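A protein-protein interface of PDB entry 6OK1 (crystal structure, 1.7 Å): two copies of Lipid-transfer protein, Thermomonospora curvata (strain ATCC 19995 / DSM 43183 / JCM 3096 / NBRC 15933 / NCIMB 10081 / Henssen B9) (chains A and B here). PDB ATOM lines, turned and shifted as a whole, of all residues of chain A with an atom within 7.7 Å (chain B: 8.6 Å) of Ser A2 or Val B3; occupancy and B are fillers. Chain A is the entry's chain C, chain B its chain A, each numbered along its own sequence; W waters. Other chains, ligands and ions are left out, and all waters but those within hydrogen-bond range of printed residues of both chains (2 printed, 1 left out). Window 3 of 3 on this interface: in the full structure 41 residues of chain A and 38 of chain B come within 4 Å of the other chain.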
ATOM      1  N   SER A   2      22.264   5.434 -18.048  1.00  0.00           N
ATOM      2  CA  SER A   2      22.373   6.690 -18.781  1.00  0.00           C
ATOM      3  C   SER A   2      23.512   6.620 -19.783  1.00  0.00           C
ATOM      4  O   SER A   2      24.362   7.503 -19.836  1.00  0.00           O
ATOM      5  CB  SER A   2      22.591   7.861 -17.828  1.00  0.00           C
ATOM      6  OG  SER A   2      21.464   8.042 -16.981  1.00  0.00           O
ATOM      7  N   VAL A   3      23.536   5.544 -20.564  1.00  0.00           N
ATOM      8  CA  VAL A   3      24.464   5.452 -21.681  1.00  0.00           C
ATOM      9  C   VAL A   3      24.000   6.397 -22.778  1.00  0.00           C
ATOM     10  O   VAL A   3      22.820   6.398 -23.156  1.00  0.00           O
ATOM     11  CB  VAL A   3      24.536   4.010 -22.200  1.00  0.00           C
ATOM     12  CG1 VAL A   3      25.589   3.893 -23.323  1.00  0.00           C
ATOM     13  CG2 VAL A   3      24.841   3.063 -21.055  1.00  0.00           C
ATOM     14  N   LEU A   4      24.909   7.203 -23.285  1.00  0.00           N
ATOM     15  CA  LEU A   4      24.459   8.233 -24.224  1.00  0.00           C
ATOM     16  C   LEU A   4      24.571   7.799 -25.685  1.00  0.00           C
ATOM     17  O   LEU A   4      23.595   7.918 -26.434  1.00  0.00           O
ATOM     18  CB  LEU A   4      25.230   9.531 -24.004  1.00  0.00           C
ATOM     19  CG  LEU A   4      24.878  10.675 -24.961  1.00  0.00           C
ATOM     20  CD1 LEU A   4      23.461  11.144 -24.771  1.00  0.00           C
ATOM     21  CD2 LEU A   4      25.860  11.837 -24.790  1.00  0.00           C
ATOM     22  N   PRO A   5      25.721   7.311 -26.148  1.00  0.00           N
ATOM     23  CA  PRO A   5      25.839   6.996 -27.584  1.00  0.00           C
ATOM     24  C   PRO A   5      24.850   5.933 -28.022  1.00  0.00           C
ATOM     25  O   PRO A   5      24.823   4.823 -27.484  1.00  0.00           O
ATOM     26  CB  PRO A   5      27.286   6.505 -27.723  1.00  0.00           C
ATOM     27  CG  PRO A   5      27.999   7.141 -26.529  1.00  0.00           C
ATOM     28  CD  PRO A   5      26.977   7.042 -25.427  1.00  0.00           C
ATOM     29  N   ALA A   7      21.647   6.000 -27.752  1.00  0.00           N
ATOM     30  CA  ALA A   7      20.437   5.914 -26.942  1.00  0.00           C
ATOM     31  C   ALA A   7      19.280   6.683 -27.562  1.00  0.00           C
ATOM     32  O   ALA A   7      18.109   6.316 -27.378  1.00  0.00           O
ATOM     33  CB  ALA A   7      20.728   6.445 -25.533  1.00  0.00           C
ATOM     34  N   MET A  95      20.761  13.853 -24.360  1.00  0.00           N
ATOM     35  CA  MET A  95      21.051  13.710 -22.942  1.00  0.00           C
ATOM     36  C   MET A  95      19.780  13.638 -22.114  1.00  0.00           C
ATOM     37  O   MET A  95      19.703  12.846 -21.164  1.00  0.00           O
ATOM     38  CB  MET A  95      21.921  14.875 -22.489  1.00  0.00           C
ATOM     39  CG  MET A  95      23.263  14.872 -23.172  1.00  0.00           C
ATOM     40  SD  MET A  95      24.293  16.342 -22.875  1.00  0.00           S
ATOM     41  CE  MET A  95      23.362  17.795 -23.216  1.00  0.00           C
ATOM     42  N   VAL A  97      16.893  12.531 -23.196  1.00  0.00           N
ATOM     43  CA  VAL A  97      16.291  11.222 -23.489  1.00  0.00           C
ATOM     44  C   VAL A  97      17.050  10.115 -22.766  1.00  0.00           C
ATOM     45  O   VAL A  97      16.459   9.257 -22.096  1.00  0.00           O
ATOM     46  CB  VAL A  97      16.239  10.991 -25.013  1.00  0.00           C
ATOM     47  CG1 VAL A  97      15.892   9.517 -25.358  1.00  0.00           C
ATOM     48  CG2 VAL A  97      15.203  11.939 -25.650  1.00  0.00           C
ATOM     49  N   ALA A  98      18.372  10.156 -22.839  1.00  0.00           N
ATOM     50  CA  ALA A  98      19.179   9.095 -22.243  1.00  0.00           C
ATOM     51  C   ALA A  98      19.009   9.008 -20.730  1.00  0.00           C
ATOM     52  O   ALA A  98      19.123   7.909 -20.163  1.00  0.00           O
ATOM     53  CB  ALA A  98      20.642   9.301 -22.611  1.00  0.00           C
ATOM     54  N   THR A  99      18.723  10.130 -20.060  1.00  0.00           N
ATOM     55  CA  THR A  99      18.582  10.184 -18.613  1.00  0.00           C
ATOM     56  C   THR A  99      17.147  10.031 -18.150  1.00  0.00           C
ATOM     57  O   THR A  99      16.907  10.024 -16.941  1.00  0.00           O
ATOM     58  CB  THR A  99      19.135  11.502 -18.054  1.00  0.00           C
ATOM     59  OG1 THR A  99      18.497  12.633 -18.687  1.00  0.00           O
ATOM     60  CG2 THR A  99      20.628  11.553 -18.258  1.00  0.00           C
ATOM     61  N   GLY A 100      16.193   9.942 -19.073  1.00  0.00           N
ATOM     62  CA  GLY A 100      14.797   9.787 -18.697  1.00  0.00           C
ATOM     63  C   GLY A 100      14.111  11.077 -18.329  1.00  0.00           C
ATOM     64  O   GLY A 100      12.958  11.056 -17.867  1.00  0.00           O
ATOM     65  N   VAL B   3      21.499   6.339 -15.555  1.00  0.00           N
ATOM     66  CA  VAL B   3      20.622   6.524 -14.412  1.00  0.00           C
ATOM     67  C   VAL B   3      20.960   7.880 -13.836  1.00  0.00           C
ATOM     68  O   VAL B   3      22.107   8.154 -13.521  1.00  0.00           O
ATOM     69  CB  VAL B   3      20.790   5.425 -13.347  1.00  0.00           C
ATOM     70  CG1 VAL B   3      19.531   5.353 -12.458  1.00  0.00           C
ATOM     71  CG2 VAL B   3      21.101   4.069 -13.966  1.00  0.00           C
ATOM     72  N   LEU B   4      19.971   8.738 -13.720  1.00  0.00           N
ATOM     73  CA  LEU B   4      20.253  10.091 -13.257  1.00  0.00           C
ATOM     74  C   LEU B   4      20.163  10.233 -11.741  1.00  0.00           C
ATOM     75  O   LEU B   4      21.081  10.798 -11.127  1.00  0.00           O
ATOM     76  CB  LEU B   4      19.310  11.076 -13.947  1.00  0.00           C
ATOM     77  CG  LEU B   4      19.414  12.536 -13.501  1.00  0.00           C
ATOM     78  CD1 LEU B   4      20.771  13.079 -13.850  1.00  0.00           C
ATOM     79  CD2 LEU B   4      18.299  13.358 -14.140  1.00  0.00           C
ATOM     80  N   PRO B   5      19.093   9.773 -11.084  1.00  0.00           N
ATOM     81  CA  PRO B   5      18.946  10.095  -9.661  1.00  0.00           C
ATOM     82  C   PRO B   5      20.078   9.499  -8.847  1.00  0.00           C
ATOM     83  O   PRO B   5      20.392   8.310  -8.963  1.00  0.00           O
ATOM     84  CB  PRO B   5      17.588   9.491  -9.291  1.00  0.00           C
ATOM     85  CG  PRO B   5      16.850   9.462 -10.579  1.00  0.00           C
ATOM     86  CD  PRO B   5      17.894   9.091 -11.597  1.00  0.00           C
ATOM     87  N   GLY B   6      20.697  10.339  -8.026  1.00  0.00           N
ATOM     88  CA  GLY B   6      21.801   9.926  -7.192  1.00  0.00           C
ATOM     89  C   GLY B   6      23.127   9.790  -7.899  1.00  0.00           C
ATOM     90  O   GLY B   6      24.138   9.527  -7.237  1.00  0.00           O
ATOM     91  N   ALA B   7      23.166   9.978  -9.219  1.00  0.00           N
ATOM     92  CA  ALA B   7      24.406   9.757  -9.965  1.00  0.00           C
ATOM     93  C   ALA B   7      25.416  10.868  -9.730  1.00  0.00           C
ATOM     94  O   ALA B   7      26.631  10.636  -9.822  1.00  0.00           O
ATOM     95  CB  ALA B   7      24.100   9.638 -11.456  1.00  0.00           C
ATOM     96  N   ALA B   8      24.944  12.081  -9.459  1.00  0.00           N
ATOM     97  CA  ALA B   8      25.809  13.233  -9.290  1.00  0.00           C
ATOM     98  C   ALA B   8      25.560  13.884  -7.942  1.00  0.00           C
ATOM     99  O   ALA B   8      24.523  13.680  -7.300  1.00  0.00           O
ATOM    100  CB  ALA B   8      25.561  14.279 -10.394  1.00  0.00           C
ATOM    101  N   ALA B  94      24.043  17.697 -13.531  1.00  0.00           N
ATOM    102  CA  ALA B  94      23.834  16.293 -13.173  1.00  0.00           C
ATOM    103  C   ALA B  94      23.650  15.420 -14.405  1.00  0.00           C
ATOM    104  O   ALA B  94      24.140  14.290 -14.452  1.00  0.00           O
ATOM    105  CB  ALA B  94      22.619  16.167 -12.254  1.00  0.00           C
ATOM    106  N   MET B  95      22.914  15.917 -15.393  1.00  0.00           N
ATOM    107  CA  MET B  95      22.714  15.200 -16.647  1.00  0.00           C
ATOM    108  C   MET B  95      24.029  15.005 -17.390  1.00  0.00           C
ATOM    109  O   MET B  95      24.291  13.933 -17.951  1.00  0.00           O
ATOM    110  CB  MET B  95      21.719  15.997 -17.491  1.00  0.00           C
ATOM    111  CG  MET B  95      21.260  15.388 -18.784  1.00  0.00           C
ATOM    112  SD  MET B  95      20.231  16.529 -19.753  1.00  0.00           S
ATOM    113  CE  MET B  95      19.578  17.618 -18.486  1.00  0.00           C
ATOM    114  N   ALA B  96      24.860  16.048 -17.434  1.00  0.00           N
ATOM    115  CA  ALA B  96      26.141  15.936 -18.130  1.00  0.00           C
ATOM    116  C   ALA B  96      27.052  14.938 -17.429  1.00  0.00           C
ATOM    117  O   ALA B  96      27.812  14.202 -18.084  1.00  0.00           O
ATOM    118  CB  ALA B  96      26.823  17.306 -18.213  1.00  0.00           C
ATOM    119  N   VAL B  97      26.997  14.905 -16.096  1.00  0.00           N
ATOM    120  CA  VAL B  97      27.801  13.946 -15.341  1.00  0.00           C
ATOM    121  C   VAL B  97      27.281  12.528 -15.571  1.00  0.00           C
ATOM    122  O   VAL B  97      28.054  11.600 -15.852  1.00  0.00           O
ATOM    123  CB  VAL B  97      27.809  14.319 -13.851  1.00  0.00           C
ATOM    124  CG1 VAL B  97      28.374  13.172 -12.976  1.00  0.00           C
ATOM    125  CG2 VAL B  97      28.624  15.586 -13.630  1.00  0.00           C
ATOM    126  N   ALA B  98      25.963  12.345 -15.466  1.00  0.00           N
ATOM    127  CA  ALA B  98      25.378  11.015 -15.578  1.00  0.00           C
ATOM    128  C   ALA B  98      25.642  10.386 -16.942  1.00  0.00           C
ATOM    129  O   ALA B  98      25.791   9.156 -17.046  1.00  0.00           O
ATOM    130  CB  ALA B  98      23.874  11.083 -15.312  1.00  0.00           C
ATOM    131  N   THR B  99      25.691  11.195 -17.999  1.00  0.00           N
ATOM    132  CA  THR B  99      25.888  10.686 -19.350  1.00  0.00           C
ATOM    133  C   THR B  99      27.357  10.620 -19.747  1.00  0.00           C
ATOM    134  O   THR B  99      27.657  10.188 -20.864  1.00  0.00           O
ATOM    135  CB  THR B  99      25.142  11.549 -20.373  1.00  0.00           C
ATOM    136  OG1 THR B  99      25.612  12.908 -20.266  1.00  0.00           O
ATOM    137  CG2 THR B  99      23.629  11.465 -20.154  1.00  0.00           C
ATOM    138  N   GLY B 100      28.264  11.049 -18.880  1.00  0.00           N
ATOM    139  CA  GLY B 100      29.684  11.021 -19.187  1.00  0.00           C
ATOM    140  C   GLY B 100      30.168  12.133 -20.082  1.00  0.00           C
ATOM    141  O   GLY B 100      31.311  12.106 -20.540  1.00  0.00           O
ATOM    142  N   ILE B 101      29.343  13.130 -20.351  1.00  0.00           N
ATOM    143  CA  ILE B 101      29.783  14.253 -21.171  1.00  0.00           C
ATOM    144  C   ILE B 101      30.816  15.089 -20.419  1.00  0.00           C
ATOM    145  O   ILE B 101      31.791  15.585 -21.001  1.00  0.00           O
ATOM    146  CB  ILE B 101      28.561  15.092 -21.587  1.00  0.00           C
ATOM    147  CG1 ILE B 101      27.735  14.337 -22.637  1.00  0.00           C
ATOM    148  CG2 ILE B 101      28.985  16.466 -22.102  1.00  0.00           C
ATOM    149  CD1 ILE B 101      28.513  14.015 -23.959  1.00  0.00           C
ATOM    150  N   ILE B 242      22.372  14.536  -5.635  1.00  0.00           N
ATOM    151  CA  ILE B 242      21.258  15.064  -6.404  1.00  0.00           C
ATOM    152  C   ILE B 242      20.326  13.880  -6.660  1.00  0.00           C
ATOM    153  O   ILE B 242      20.425  13.176  -7.669  1.00  0.00           O
ATOM    154  CB  ILE B 242      21.737  15.750  -7.680  1.00  0.00           C
ATOM    155  CG1 ILE B 242      22.648  16.927  -7.302  1.00  0.00           C
ATOM    156  CG2 ILE B 242      20.577  16.256  -8.468  1.00  0.00           C
ATOM    157  CD1 ILE B 242      23.573  17.385  -8.434  1.00  0.00           C
ATOM    158  N   TRP B 243      19.391  13.681  -5.730  1.00  0.00           N
ATOM    159  CA  TRP B 243      18.410  12.603  -5.825  1.00  0.00           C
ATOM    160  C   TRP B 243      17.225  12.952  -6.708  1.00  0.00           C
ATOM    161  O   TRP B 243      16.610  12.053  -7.299  1.00  0.00           O
ATOM    162  CB  TRP B 243      17.891  12.230  -4.446  1.00  0.00           C
ATOM    163  CG  TRP B 243      18.839  11.323  -3.749  1.00  0.00           C
ATOM    164  CD1 TRP B 243      19.518  11.577  -2.610  1.00  0.00           C
ATOM    165  CD2 TRP B 243      19.254  10.016  -4.190  1.00  0.00           C
ATOM    166  NE1 TRP B 243      20.314  10.493  -2.271  1.00  0.00           N
ATOM    167  CE2 TRP B 243      20.173   9.527  -3.232  1.00  0.00           C
ATOM    168  CE3 TRP B 243      18.926   9.212  -5.281  1.00  0.00           C
ATOM    169  CZ2 TRP B 243      20.770   8.284  -3.345  1.00  0.00           C
ATOM    170  CZ3 TRP B 243      19.521   7.959  -5.386  1.00  0.00           C
ATOM    171  CH2 TRP B 243      20.437   7.517  -4.427  1.00  0.00           C
ATOM    172  N   GLN B 280      11.691  10.513  -9.114  1.00  0.00           N
ATOM    173  CA  GLN B 280      13.109  10.256  -9.357  1.00  0.00           C
ATOM    174  C   GLN B 280      13.775   9.693  -8.110  1.00  0.00           C
ATOM    175  O   GLN B 280      14.561   8.739  -8.176  1.00  0.00           O
ATOM    176  CB  GLN B 280      13.824  11.543  -9.765  1.00  0.00           C
ATOM    177  CG  GLN B 280      13.526  12.014 -11.173  1.00  0.00           C
ATOM    178  CD  GLN B 280      14.045  13.416 -11.395  1.00  0.00           C
ATOM    179  OE1 GLN B 280      14.614  14.006 -10.493  1.00  0.00           O
ATOM    180  NE2 GLN B 280      13.845  13.954 -12.582  1.00  0.00           N
HETATM  181  O   HOH W   1      17.638   8.033 -15.156  1.00  0.00           O
HETATM  182  O   HOH W   2      27.470   7.615 -21.857  1.00  0.00           O
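The side-chain hydroxyl (OG) of Ser A2 lies close to the backbone NH (N) of Val B3 (2.2 Å).
The backbone carbonyl oxygen (O) of Ala B96 is in hydrogen-bond range of the backbone NH (N) of Ile B101. The backbone carbonyl oxygen of Ala B96 lies within hydrogen-bond range of the side-chain hydroxyl of Thr B99, at 3.4 Å. OG1 of Thr A99 is in hydrogen-bond range of O of Met A95, 2.8 Å away. The backbone carbonyl oxygen (O) of Met B95 is in hydrogen-bond range of the side-chain hydroxyl (OG1) of Thr B99.
Among the printed residues, merely in contact across the chains: Leu A4 with Ile B101, Ser A2 with Ala B98, Thr A99 with Thr B99, Ser A2 with Thr B99, Met A95 with Met B95, Ser A2 with Leu B4, Thr A99 with Met B95, Thr A99 with Leu B4 and Met A95 with Ile B101.
Ser A2 touches just these residues of chain B: Val B3 (2.2 Å), Leu B4 (3.7 Å), Ala B98 (3.5 Å) and Thr B99 (3.6 Å). Printed residues of chain B within 4 Å of Leu A4: Ile B101 (3.5 Å). Of the printed residues of chain B, Met A95 touches Met B95 and Ile B101. Val B3 touches one residue of chain A. Printed residues of chain A within 4 Å of Met B95: Met A95 (3.6 Å) and Thr A99 (3.9 Å). Of the printed residues of chain A, Ala B98 touches Ser A2 (3.5 Å). Of the printed residues of chain A, Ile B101 touches Leu A4 (3.5 Å) and Met A95 (3.99 Å). The nearest residue of chain A that does not touch Val B3 is Ala A98 (5.4 Å). The nearest printed residue of chain A that does not touch Ile B101 is Pro A5 (7.3 Å).
Of the 10 printed residues of chain A, 4 touch a printed residue of chain B. Hydrophobic or aromatic side chains of chain A that line the printed part of chain B: Leu A4 and Met A95. Of the 17 printed residues of chain B, 6 touch a printed residue of chain A. Hydrophobic or aromatic side chains of chain B within 4 Å of the printed part of chain A: Leu B4, Met B95 and Ile B101. Among the printed residues, 10 pairs touch across the chains.
Met A95 touches its own counterpart, Met B95. Thr A99 touches Leu B4, but with the chains exchanged Leu A4 does not touch Thr B99 (4.02 Å). Thr A99 touches Met B95, but with the chains exchanged Met A95 does not touch Thr B99 (4.2 Å). Thr B99 touches its own counterpart, Thr A99.
Water W2 bridges O of Thr B99 (2.8 Å) and N of Leu A4 (3.0 Å). Water W1 bridges the backbone carbonyl oxygen (O) of Thr A99 (2.8 Å) and the backbone NH (N) of Leu B4 (2.8 Å).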
